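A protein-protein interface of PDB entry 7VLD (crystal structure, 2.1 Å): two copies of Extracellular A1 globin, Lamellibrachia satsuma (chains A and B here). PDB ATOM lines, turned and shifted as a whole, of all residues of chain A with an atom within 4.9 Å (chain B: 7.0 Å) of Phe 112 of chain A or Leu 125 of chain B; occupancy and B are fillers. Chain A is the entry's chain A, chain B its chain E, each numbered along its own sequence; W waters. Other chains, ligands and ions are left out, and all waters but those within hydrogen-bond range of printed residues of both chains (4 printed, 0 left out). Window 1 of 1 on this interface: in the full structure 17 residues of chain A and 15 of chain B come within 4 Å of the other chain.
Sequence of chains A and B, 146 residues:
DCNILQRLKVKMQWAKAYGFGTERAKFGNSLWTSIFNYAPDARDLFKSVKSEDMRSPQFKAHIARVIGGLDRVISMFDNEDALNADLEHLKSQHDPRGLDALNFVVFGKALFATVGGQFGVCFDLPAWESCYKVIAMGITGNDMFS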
ATOM      1  N   TYR A  38     -16.986 -17.214  10.454  1.00  0.00           N
ATOM      2  CA  TYR A  38     -15.824 -17.147   9.574  1.00  0.00           C
ATOM      3  C   TYR A  38     -14.613 -16.558  10.291  1.00  0.00           C
ATOM      4  O   TYR A  38     -13.476 -16.963  10.013  1.00  0.00           O
ATOM      5  CB  TYR A  38     -16.138 -16.316   8.328  1.00  0.00           C
ATOM      6  CG  TYR A  38     -17.082 -16.967   7.338  1.00  0.00           C
ATOM      7  CD1 TYR A  38     -17.503 -18.282   7.498  1.00  0.00           C
ATOM      8  CD2 TYR A  38     -17.542 -16.262   6.233  1.00  0.00           C
ATOM      9  CE1 TYR A  38     -18.364 -18.871   6.585  1.00  0.00           C
ATOM     10  CE2 TYR A  38     -18.399 -16.841   5.319  1.00  0.00           C
ATOM     11  CZ  TYR A  38     -18.809 -18.144   5.498  1.00  0.00           C
ATOM     12  OH  TYR A  38     -19.663 -18.714   4.582  1.00  0.00           O
ATOM     13  N   GLY A 108     -17.749  -9.758   2.878  1.00  0.00           N
ATOM     14  CA  GLY A 108     -18.230 -10.070   1.542  1.00  0.00           C
ATOM     15  C   GLY A 108     -18.507 -11.548   1.343  1.00  0.00           C
ATOM     16  O   GLY A 108     -19.517 -11.923   0.744  1.00  0.00           O
ATOM     17  N   LYS A 109     -17.618 -12.408   1.845  1.00  0.00           N
ATOM     18  CA  LYS A 109     -17.831 -13.844   1.699  1.00  0.00           C
ATOM     19  C   LYS A 109     -19.036 -14.309   2.507  1.00  0.00           C
ATOM     20  O   LYS A 109     -19.775 -15.198   2.071  1.00  0.00           O
ATOM     21  CB  LYS A 109     -16.566 -14.602   2.101  1.00  0.00           C
ATOM     22  CG  LYS A 109     -15.424 -14.381   1.122  1.00  0.00           C
ATOM     23  CD  LYS A 109     -14.149 -15.098   1.521  1.00  0.00           C
ATOM     24  CE  LYS A 109     -13.048 -14.814   0.508  1.00  0.00           C
ATOM     25  NZ  LYS A 109     -11.738 -15.390   0.911  1.00  0.00           N
ATOM     26  N   ALA A 110     -19.260 -13.712   3.681  1.00  0.00           N
ATOM     27  CA  ALA A 110     -20.468 -14.022   4.435  1.00  0.00           C
ATOM     28  C   ALA A 110     -21.712 -13.482   3.740  1.00  0.00           C
ATOM     29  O   ALA A 110     -22.778 -14.104   3.809  1.00  0.00           O
ATOM     30  CB  ALA A 110     -20.363 -13.466   5.853  1.00  0.00           C
ATOM     31  N   LEU A 111     -21.593 -12.335   3.066  1.00  0.00           N
ATOM     32  CA  LEU A 111     -22.713 -11.798   2.298  1.00  0.00           C
ATOM     33  C   LEU A 111     -23.047 -12.702   1.115  1.00  0.00           C
ATOM     34  O   LEU A 111     -24.220 -12.991   0.854  1.00  0.00           O
ATOM     35  CB  LEU A 111     -22.386 -10.382   1.821  1.00  0.00           C
ATOM     36  CG  LEU A 111     -23.388  -9.729   0.866  1.00  0.00           C
ATOM     37  CD1 LEU A 111     -24.668  -9.339   1.594  1.00  0.00           C
ATOM     38  CD2 LEU A 111     -22.764  -8.526   0.167  1.00  0.00           C
ATOM     39  N   PHE A 112     -22.022 -13.155   0.387  1.00  0.00           N
ATOM     40  CA  PHE A 112     -22.252 -14.040  -0.751  1.00  0.00           C
ATOM     41  C   PHE A 112     -22.928 -15.333  -0.307  1.00  0.00           C
ATOM     42  O   PHE A 112     -23.898 -15.787  -0.927  1.00  0.00           O
ATOM     43  CB  PHE A 112     -20.932 -14.351  -1.464  1.00  0.00           C
ATOM     44  CG  PHE A 112     -20.153 -13.132  -1.882  1.00  0.00           C
ATOM     45  CD1 PHE A 112     -20.794 -11.936  -2.167  1.00  0.00           C
ATOM     46  CD2 PHE A 112     -18.772 -13.187  -1.988  1.00  0.00           C
ATOM     47  CE1 PHE A 112     -20.072 -10.819  -2.545  1.00  0.00           C
ATOM     48  CE2 PHE A 112     -18.045 -12.072  -2.367  1.00  0.00           C
ATOM     49  CZ  PHE A 112     -18.697 -10.888  -2.645  1.00  0.00           C
ATOM     50  N   ALA A 113     -22.428 -15.939   0.773  1.00  0.00           N
ATOM     51  CA  ALA A 113     -23.014 -17.183   1.265  1.00  0.00           C
ATOM     52  C   ALA A 113     -24.459 -16.981   1.700  1.00  0.00           C
ATOM     53  O   ALA A 113     -25.302 -17.867   1.514  1.00  0.00           O
ATOM     54  CB  ALA A 113     -22.180 -17.736   2.420  1.00  0.00           C
ATOM     55  N   THR A 114     -24.767 -15.819   2.276  1.00  0.00           N
ATOM     56  CA  THR A 114     -26.118 -15.576   2.767  1.00  0.00           C
ATOM     57  C   THR A 114     -27.079 -15.247   1.629  1.00  0.00           C
ATOM     58  O   THR A 114     -28.194 -15.779   1.587  1.00  0.00           O
ATOM     59  CB  THR A 114     -26.107 -14.454   3.806  1.00  0.00           C
ATOM     60  OG1 THR A 114     -25.126 -14.748   4.810  1.00  0.00           O
ATOM     61  CG2 THR A 114     -27.467 -14.336   4.469  1.00  0.00           C
ATOM     62  N   VAL A 115     -26.671 -14.381   0.699  1.00  0.00           N
ATOM     63  CA  VAL A 115     -27.524 -14.074  -0.447  1.00  0.00           C
ATOM     64  C   VAL A 115     -27.692 -15.307  -1.326  1.00  0.00           C
ATOM     65  O   VAL A 115     -28.809 -15.658  -1.726  1.00  0.00           O
ATOM     66  CB  VAL A 115     -26.956 -12.889  -1.248  1.00  0.00           C
ATOM     67  CG1 VAL A 115     -27.773 -12.675  -2.518  1.00  0.00           C
ATOM     68  CG2 VAL A 115     -26.944 -11.626  -0.403  1.00  0.00           C
ATOM     69  N   GLY A 116     -26.585 -15.984  -1.639  1.00  0.00           N
ATOM     70  CA  GLY A 116     -26.663 -17.160  -2.491  1.00  0.00           C
ATOM     71  C   GLY A 116     -27.465 -18.286  -1.870  1.00  0.00           C
ATOM     72  O   GLY A 116     -28.223 -18.975  -2.558  1.00  0.00           O
ATOM     73  N   GLY A 117     -27.310 -18.490  -0.560  1.00  0.00           N
ATOM     74  CA  GLY A 117     -28.087 -19.512   0.117  1.00  0.00           C
ATOM     75  C   GLY A 117     -29.569 -19.207   0.149  1.00  0.00           C
ATOM     76  O   GLY A 117     -30.395 -20.125   0.142  1.00  0.00           O
ATOM     77  N   PHE A 123     -27.752 -17.763  -8.247  1.00  0.00           N
ATOM     78  CA  PHE A 123     -26.926 -16.711  -7.671  1.00  0.00           C
ATOM     79  C   PHE A 123     -25.706 -16.465  -8.551  1.00  0.00           C
ATOM     80  O   PHE A 123     -25.022 -17.406  -8.963  1.00  0.00           O
ATOM     81  CB  PHE A 123     -26.516 -17.122  -6.255  1.00  0.00           C
ATOM     82  CG  PHE A 123     -25.576 -16.170  -5.574  1.00  0.00           C
ATOM     83  CD1 PHE A 123     -26.008 -14.927  -5.149  1.00  0.00           C
ATOM     84  CD2 PHE A 123     -24.268 -16.547  -5.314  1.00  0.00           C
ATOM     85  CE1 PHE A 123     -25.143 -14.063  -4.503  1.00  0.00           C
ATOM     86  CE2 PHE A 123     -23.399 -15.688  -4.670  1.00  0.00           C
ATOM     87  CZ  PHE A 123     -23.837 -14.443  -4.264  1.00  0.00           C
ATOM     88  N   LEU A 125     -22.372 -15.350  -8.502  1.00  0.00           N
ATOM     89  CA  LEU A 125     -21.225 -15.053  -7.647  1.00  0.00           C
ATOM     90  C   LEU A 125     -20.206 -14.118  -8.294  1.00  0.00           C
ATOM     91  O   LEU A 125     -19.744 -13.193  -7.602  1.00  0.00           O
ATOM     92  CB  LEU A 125     -20.565 -16.365  -7.201  1.00  0.00           C
ATOM     93  CG  LEU A 125     -19.318 -16.259  -6.321  1.00  0.00           C
ATOM     94  CD1 LEU A 125     -19.610 -15.467  -5.054  1.00  0.00           C
ATOM     95  CD2 LEU A 125     -18.786 -17.643  -5.980  1.00  0.00           C
ATOM     96  N   TRP A 128     -21.455 -10.630  -7.918  1.00  0.00           N
ATOM     97  CA  TRP A 128     -21.469 -10.163  -6.534  1.00  0.00           C
ATOM     98  C   TRP A 128     -20.060  -9.882  -6.025  1.00  0.00           C
ATOM     99  O   TRP A 128     -19.849  -8.921  -5.278  1.00  0.00           O
ATOM    100  CB  TRP A 128     -22.177 -11.183  -5.644  1.00  0.00           C
ATOM    101  CG  TRP A 128     -23.667 -11.031  -5.656  1.00  0.00           C
ATOM    102  CD1 TRP A 128     -24.543 -11.595  -6.537  1.00  0.00           C
ATOM    103  CD2 TRP A 128     -24.455 -10.253  -4.749  1.00  0.00           C
ATOM    104  NE1 TRP A 128     -25.828 -11.222  -6.231  1.00  0.00           N
ATOM    105  CE2 TRP A 128     -25.802 -10.396  -5.138  1.00  0.00           C
ATOM    106  CE3 TRP A 128     -24.153  -9.450  -3.644  1.00  0.00           C
ATOM    107  CZ2 TRP A 128     -26.844  -9.766  -4.461  1.00  0.00           C
ATOM    108  CZ3 TRP A 128     -25.190  -8.826  -2.975  1.00  0.00           C
ATOM    109  CH2 TRP A 128     -26.519  -8.988  -3.385  1.00  0.00           C
ATOM    110  N   GLU A 129     -19.085 -10.707  -6.416  1.00  0.00           N
ATOM    111  CA  GLU A 129     -17.700 -10.432  -6.043  1.00  0.00           C
ATOM    112  C   GLU A 129     -17.219  -9.115  -6.642  1.00  0.00           C
ATOM    113  O   GLU A 129     -16.541  -8.329  -5.971  1.00  0.00           O
ATOM    114  CB  GLU A 129     -16.794 -11.581  -6.488  1.00  0.00           C
ATOM    115  CG  GLU A 129     -17.034 -12.898  -5.766  1.00  0.00           C
ATOM    116  CD  GLU A 129     -16.115 -13.997  -6.260  1.00  0.00           C
ATOM    117  OE1 GLU A 129     -15.739 -13.963  -7.450  1.00  0.00           O
ATOM    118  OE2 GLU A 129     -15.761 -14.891  -5.461  1.00  0.00           O
ATOM    119  N   TYR A 132     -19.334  -6.088  -4.976  1.00  0.00           N
ATOM    120  CA  TYR A 132     -18.995  -5.859  -3.574  1.00  0.00           C
ATOM    121  C   TYR A 132     -17.642  -5.173  -3.438  1.00  0.00           C
ATOM    122  O   TYR A 132     -17.448  -4.372  -2.515  1.00  0.00           O
ATOM    123  CB  TYR A 132     -18.996  -7.163  -2.775  1.00  0.00           C
ATOM    124  CG  TYR A 132     -18.548  -6.946  -1.345  1.00  0.00           C
ATOM    125  CD1 TYR A 132     -19.398  -6.359  -0.416  1.00  0.00           C
ATOM    126  CD2 TYR A 132     -17.267  -7.291  -0.933  1.00  0.00           C
ATOM    127  CE1 TYR A 132     -18.991  -6.139   0.888  1.00  0.00           C
ATOM    128  CE2 TYR A 132     -16.850  -7.074   0.369  1.00  0.00           C
ATOM    129  CZ  TYR A 132     -17.718  -6.498   1.275  1.00  0.00           C
ATOM    130  OH  TYR A 132     -17.309  -6.280   2.572  1.00  0.00           O
ATOM    131  N   GLN B  13     -21.175 -30.724   3.357  1.00  0.00           N
ATOM    132  CA  GLN B  13     -22.055 -29.858   2.580  1.00  0.00           C
ATOM    133  C   GLN B  13     -22.238 -30.367   1.155  1.00  0.00           C
ATOM    134  O   GLN B  13     -23.301 -30.159   0.561  1.00  0.00           O
ATOM    135  CB  GLN B  13     -21.510 -28.429   2.583  1.00  0.00           C
ATOM    136  CG  GLN B  13     -21.432 -27.819   3.978  1.00  0.00           C
ATOM    137  CD  GLN B  13     -21.012 -26.362   3.969  1.00  0.00           C
ATOM    138  OE1 GLN B  13     -20.504 -25.852   2.969  1.00  0.00           O
ATOM    139  NE2 GLN B  13     -21.227 -25.682   5.089  1.00  0.00           N
ATOM    140  N   GLY B 108     -14.922 -23.173 -10.527  1.00  0.00           N
ATOM    141  CA  GLY B 108     -15.049 -23.066  -9.084  1.00  0.00           C
ATOM    142  C   GLY B 108     -16.204 -22.182  -8.656  1.00  0.00           C
ATOM    143  O   GLY B 108     -16.957 -22.530  -7.745  1.00  0.00           O
ATOM    144  N   PHE B 112     -19.495 -23.138  -6.493  1.00  0.00           N
ATOM    145  CA  PHE B 112     -19.876 -22.490  -5.241  1.00  0.00           C
ATOM    146  C   PHE B 112     -21.321 -22.010  -5.289  1.00  0.00           C
ATOM    147  O   PHE B 112     -22.077 -22.204  -4.330  1.00  0.00           O
ATOM    148  CB  PHE B 112     -18.937 -21.320  -4.939  1.00  0.00           C
ATOM    149  CG  PHE B 112     -17.481 -21.698  -4.897  1.00  0.00           C
ATOM    150  CD1 PHE B 112     -17.088 -22.977  -4.534  1.00  0.00           C
ATOM    151  CD2 PHE B 112     -16.505 -20.772  -5.227  1.00  0.00           C
ATOM    152  CE1 PHE B 112     -15.751 -23.323  -4.502  1.00  0.00           C
ATOM    153  CE2 PHE B 112     -15.166 -21.114  -5.197  1.00  0.00           C
ATOM    154  CZ  PHE B 112     -14.788 -22.390  -4.833  1.00  0.00           C
ATOM    155  N   ALA B 113     -21.723 -21.387  -6.400  1.00  0.00           N
ATOM    156  CA  ALA B 113     -23.094 -20.900  -6.521  1.00  0.00           C
ATOM    157  C   ALA B 113     -24.101 -22.043  -6.534  1.00  0.00           C
ATOM    158  O   ALA B 113     -25.245 -21.862  -6.105  1.00  0.00           O
ATOM    159  CB  ALA B 113     -23.240 -20.049  -7.782  1.00  0.00           C
ATOM    160  N   CYS B 122     -25.833 -21.509   5.456  1.00  0.00           N
ATOM    161  CA  CYS B 122     -24.698 -21.986   6.236  1.00  0.00           C
ATOM    162  C   CYS B 122     -23.584 -22.552   5.364  1.00  0.00           C
ATOM    163  O   CYS B 122     -22.625 -23.119   5.897  1.00  0.00           O
ATOM    164  CB  CYS B 122     -25.151 -23.037   7.248  1.00  0.00           C
ATOM    165  SG  CYS B 122     -26.547 -22.529   8.270  1.00  0.00           S
ATOM    166  N   PHE B 123     -23.704 -22.422   4.044  1.00  0.00           N
ATOM    167  CA  PHE B 123     -22.631 -22.778   3.124  1.00  0.00           C
ATOM    168  C   PHE B 123     -21.349 -22.046   3.500  1.00  0.00           C
ATOM    169  O   PHE B 123     -21.356 -20.833   3.727  1.00  0.00           O
ATOM    170  CB  PHE B 123     -23.068 -22.428   1.697  1.00  0.00           C
ATOM    171  CG  PHE B 123     -22.003 -22.611   0.650  1.00  0.00           C
ATOM    172  CD1 PHE B 123     -21.614 -23.877   0.245  1.00  0.00           C
ATOM    173  CD2 PHE B 123     -21.432 -21.512   0.030  1.00  0.00           C
ATOM    174  CE1 PHE B 123     -20.653 -24.040  -0.735  1.00  0.00           C
ATOM    175  CE2 PHE B 123     -20.467 -21.669  -0.949  1.00  0.00           C
ATOM    176  CZ  PHE B 123     -20.078 -22.936  -1.331  1.00  0.00           C
ATOM    177  N   ASP B 124     -20.250 -22.793   3.588  1.00  0.00           N
ATOM    178  CA  ASP B 124     -18.966 -22.255   4.037  1.00  0.00           C
ATOM    179  C   ASP B 124     -18.152 -21.895   2.799  1.00  0.00           C
ATOM    180  O   ASP B 124     -17.366 -22.696   2.292  1.00  0.00           O
ATOM    181  CB  ASP B 124     -18.237 -23.260   4.926  1.00  0.00           C
ATOM    182  CG  ASP B 124     -17.143 -22.620   5.764  1.00  0.00           C
ATOM    183  OD1 ASP B 124     -16.485 -21.672   5.282  1.00  0.00           O
ATOM    184  OD2 ASP B 124     -16.937 -23.068   6.912  1.00  0.00           O
ATOM    185  N   LEU B 125     -18.346 -20.670   2.310  1.00  0.00           N
ATOM    186  CA  LEU B 125     -17.625 -20.225   1.119  1.00  0.00           C
ATOM    187  C   LEU B 125     -16.111 -20.221   1.303  1.00  0.00           C
ATOM    188  O   LEU B 125     -15.405 -20.693   0.397  1.00  0.00           O
ATOM    189  CB  LEU B 125     -18.141 -18.847   0.686  1.00  0.00           C
ATOM    190  CG  LEU B 125     -17.468 -18.247  -0.552  1.00  0.00           C
ATOM    191  CD1 LEU B 125     -17.579 -19.195  -1.737  1.00  0.00           C
ATOM    192  CD2 LEU B 125     -18.060 -16.884  -0.891  1.00  0.00           C
ATOM    193  N   PRO B 126     -15.545 -19.715   2.411  1.00  0.00           N
ATOM    194  CA  PRO B 126     -14.078 -19.780   2.554  1.00  0.00           C
ATOM    195  C   PRO B 126     -13.523 -21.193   2.505  1.00  0.00           C
ATOM    196  O   PRO B 126     -12.491 -21.424   1.861  1.00  0.00           O
ATOM    197  CB  PRO B 126     -13.836 -19.118   3.917  1.00  0.00           C
ATOM    198  CG  PRO B 126     -14.988 -18.203   4.093  1.00  0.00           C
ATOM    199  CD  PRO B 126     -16.155 -18.927   3.499  1.00  0.00           C
ATOM    200  N   ALA B 127     -14.183 -22.150   3.162  1.00  0.00           N
ATOM    201  CA  ALA B 127     -13.699 -23.528   3.152  1.00  0.00           C
ATOM    202  C   ALA B 127     -13.749 -24.123   1.751  1.00  0.00           C
ATOM    203  O   ALA B 127     -12.836 -24.853   1.344  1.00  0.00           O
ATOM    204  CB  ALA B 127     -14.516 -24.377   4.126  1.00  0.00           C
ATOM    205  N   TRP B 128     -14.808 -23.822   0.996  1.00  0.00           N
ATOM    206  CA  TRP B 128     -14.919 -24.346  -0.363  1.00  0.00           C
ATOM    207  C   TRP B 128     -13.886 -23.716  -1.289  1.00  0.00           C
ATOM    208  O   TRP B 128     -13.296 -24.409  -2.127  1.00  0.00           O
ATOM    209  CB  TRP B 128     -16.333 -24.124  -0.898  1.00  0.00           C
ATOM    210  CG  TRP B 128     -17.285 -25.203  -0.491  1.00  0.00           C
ATOM    211  CD1 TRP B 128     -18.002 -25.270   0.667  1.00  0.00           C
ATOM    212  CD2 TRP B 128     -17.616 -26.380  -1.237  1.00  0.00           C
ATOM    213  NE1 TRP B 128     -18.765 -26.413   0.686  1.00  0.00           N
ATOM    214  CE2 TRP B 128     -18.544 -27.113  -0.471  1.00  0.00           C
ATOM    215  CE3 TRP B 128     -17.218 -26.885  -2.479  1.00  0.00           C
ATOM    216  CZ2 TRP B 128     -19.081 -28.323  -0.906  1.00  0.00           C
ATOM    217  CZ3 TRP B 128     -17.753 -28.086  -2.909  1.00  0.00           C
ATOM    218  CH2 TRP B 128     -18.673 -28.790  -2.125  1.00  0.00           C
ATOM    219  N   GLU B 129     -13.654 -22.408  -1.156  1.00  0.00           N
ATOM    220  CA  GLU B 129     -12.631 -21.752  -1.965  1.00  0.00           C
ATOM    221  C   GLU B 129     -11.255 -22.348  -1.703  1.00  0.00           C
ATOM    222  O   GLU B 129     -10.486 -22.594  -2.641  1.00  0.00           O
ATOM    223  CB  GLU B 129     -12.622 -20.248  -1.688  1.00  0.00           C
ATOM    224  CG  GLU B 129     -13.818 -19.489  -2.244  1.00  0.00           C
ATOM    225  CD  GLU B 129     -13.797 -18.019  -1.871  1.00  0.00           C
ATOM    226  OE1 GLU B 129     -13.091 -17.663  -0.904  1.00  0.00           O
ATOM    227  OE2 GLU B 129     -14.483 -17.219  -2.543  1.00  0.00           O
ATOM    228  N   SER B 130     -10.928 -22.594  -0.432  1.00  0.00           N
ATOM    229  CA  SER B 130      -9.623 -23.153  -0.099  1.00  0.00           C
ATOM    230  C   SER B 130      -9.478 -24.577  -0.624  1.00  0.00           C
ATOM    231  O   SER B 130      -8.411 -24.955  -1.121  1.00  0.00           O
ATOM    232  CB  SER B 130      -9.408 -23.126   1.414  1.00  0.00           C
ATOM    233  OG  SER B 130      -9.495 -21.808   1.921  1.00  0.00           O
ATOM    234  N   CYS B 131     -10.532 -25.382  -0.519  1.00  0.00           N
ATOM    235  CA  CYS B 131     -10.426 -26.785  -0.890  1.00  0.00           C
ATOM    236  C   CYS B 131     -10.634 -27.026  -2.377  1.00  0.00           C
ATOM    237  O   CYS B 131     -10.081 -27.992  -2.915  1.00  0.00           O
ATOM    238  CB  CYS B 131     -11.408 -27.623  -0.076  1.00  0.00           C
ATOM    239  SG  CYS B 131     -10.899 -27.809   1.652  1.00  0.00           S
HETATM  240  O   HOH W   1     -15.578 -14.795  -2.847  1.00  0.00           O
HETATM  241  O   HOH W   2     -21.762 -19.541   6.180  1.00  0.00           O
HETATM  242  O   HOH W   3     -25.924 -19.694  -4.469  1.00  0.00           O
HETATM  243  O   HOH W   4     -15.202 -17.528  -5.074  1.00  0.00           O
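Hydrophobic or aromatic side chains of chain B that line the printed part of chain A: Phe 112, Ala 113, Leu 125 and Pro 126. Along chain B the printed residues that touch a printed residue of chain A span positions 112 to 129. Of the 16 printed residues of chain A, 7 touch a printed residue of chain B. Printed residues of chain A that touch a printed residue of chain B: Tyr 38, Lys 109, Phe 112, Ala 113, Phe 123, Leu 125 and Glu 129. Hydrophobic or aromatic side chains of chain A that line the printed part of chain B: Tyr 38, Phe 112, Ala 113 and Leu 125. Among the printed residues, Asp or Glu carboxylates within 4 Å of a Lys or Arg side-chain nitrogen of the other chain: Lys 109 of chain A with Glu 129 of chain B.
OH of Tyr 38 of chain A sits at hydrogen-bond distance from O of Phe 123 of chain B (2.8 Å). The side-chain hydroxyl (OH) of Tyr 38 of chain A is in hydrogen-bond range of the backbone NH (N) of Leu 125 of chain B (3.3 Å). The side-chain amino group (NZ) of Lys 109 of chain A is in salt-bridge range of the side-chain carboxylate (OE1) of Glu 129 of chain B, 3.2 Å away.
Phe 112 of chain A touches just one residue of chain B: Leu 125 (3.9 Å). Of chain A, only Tyr 38 (3.3 Å), Lys 109 (3.8 Å) and Phe 112 (3.9 Å) come within 4 Å of Leu 125 of chain B. Of the printed residues of chain A, Ala 113 of chain B touches Phe 123 (3.4 Å). Of the printed residues of chain B, Lys 109 of chain A touches Leu 125 and Glu 129. Printed residues of chain B within 4 Å of Phe 123 of chain A: Ala 113 (3.4 Å). Gly 108 of chain A touches none of the printed residues of chain B. Trp 128 of chain A touches none of the printed residues of chain B. The nearest residue of chain A that does not touch Leu 125 of chain B is Ala 113 of chain A (4.5 Å).
Asp 124 of chain B touches Tyr 38 of chain A (OD1 to CE1, 3.6 Å). Pro 126 of chain B touches Tyr 38 of chain A (CD to CZ, 3.4 Å). Leu 125 of chain B touches Lys 109 of chain A. Phe 112 of chain A touches Leu 125 of chain B (CB to CD2, 3.9 Å). CB of Ala 113 of chain A touches O of Phe 123 of chain B (3.5 Å). CB of Ala 113 of chain B touches O of Phe 123 of chain A, 3.4 Å away. Phe 112 of chain B touches Leu 125 of chain A. Glu 129 of chain A touches Glu 129 of chain B.
Phe 112 of chain A touches Leu 125 of chain B, and with the chains exchanged Leu 125 of chain A touches Phe 112 of chain B. Ala 113 of chain A touches Phe 123 of chain B, and with the chains exchanged Phe 123 of chain A touches Ala 113 of chain B. Glu 129 of chain A touches its own counterpart, Glu 129 of chain B. Positions printed for both chains: 108, 112, 113, 123, 125, 128 and 129.
Water W1 bridges the side-chain carboxylate of Glu 129 of chain A and the side-chain carboxylate of Glu 129 of chain B. Water W4 bridges the side-chain carboxylate of Glu 129 of chain B and the side-chain carboxylate of Glu 129 of chain A. Water W2 lies within hydrogen-bond range of the side-chain hydroxyl of Tyr 38 of chain A (2.8 Å) and the backbone carbonyl oxygen of Phe 123 of chain B (2.8 Å). Water W3 bridges the backbone carbonyl oxygen (O) of Ala 113 of chain B and the backbone carbonyl oxygen (O) of Gly 116 of chain A.
The side-chain amide oxygen (OE1) of Gln 13 of chain B is in hydrogen-bond range of the backbone NH (N) of Asp 124 of chain B. The side-chain carboxylate (OD1) of Asp 124 of chain B sits at hydrogen-bond distance from the backbone NH (N) of Ala 127 of chain B (3.2 Å). The backbone carbonyl oxygen (O) of Pro 126 of chain B is in hydrogen-bond range of the side-chain hydroxyl (OG) of Ser 130 of chain B, at 3.0 Å.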
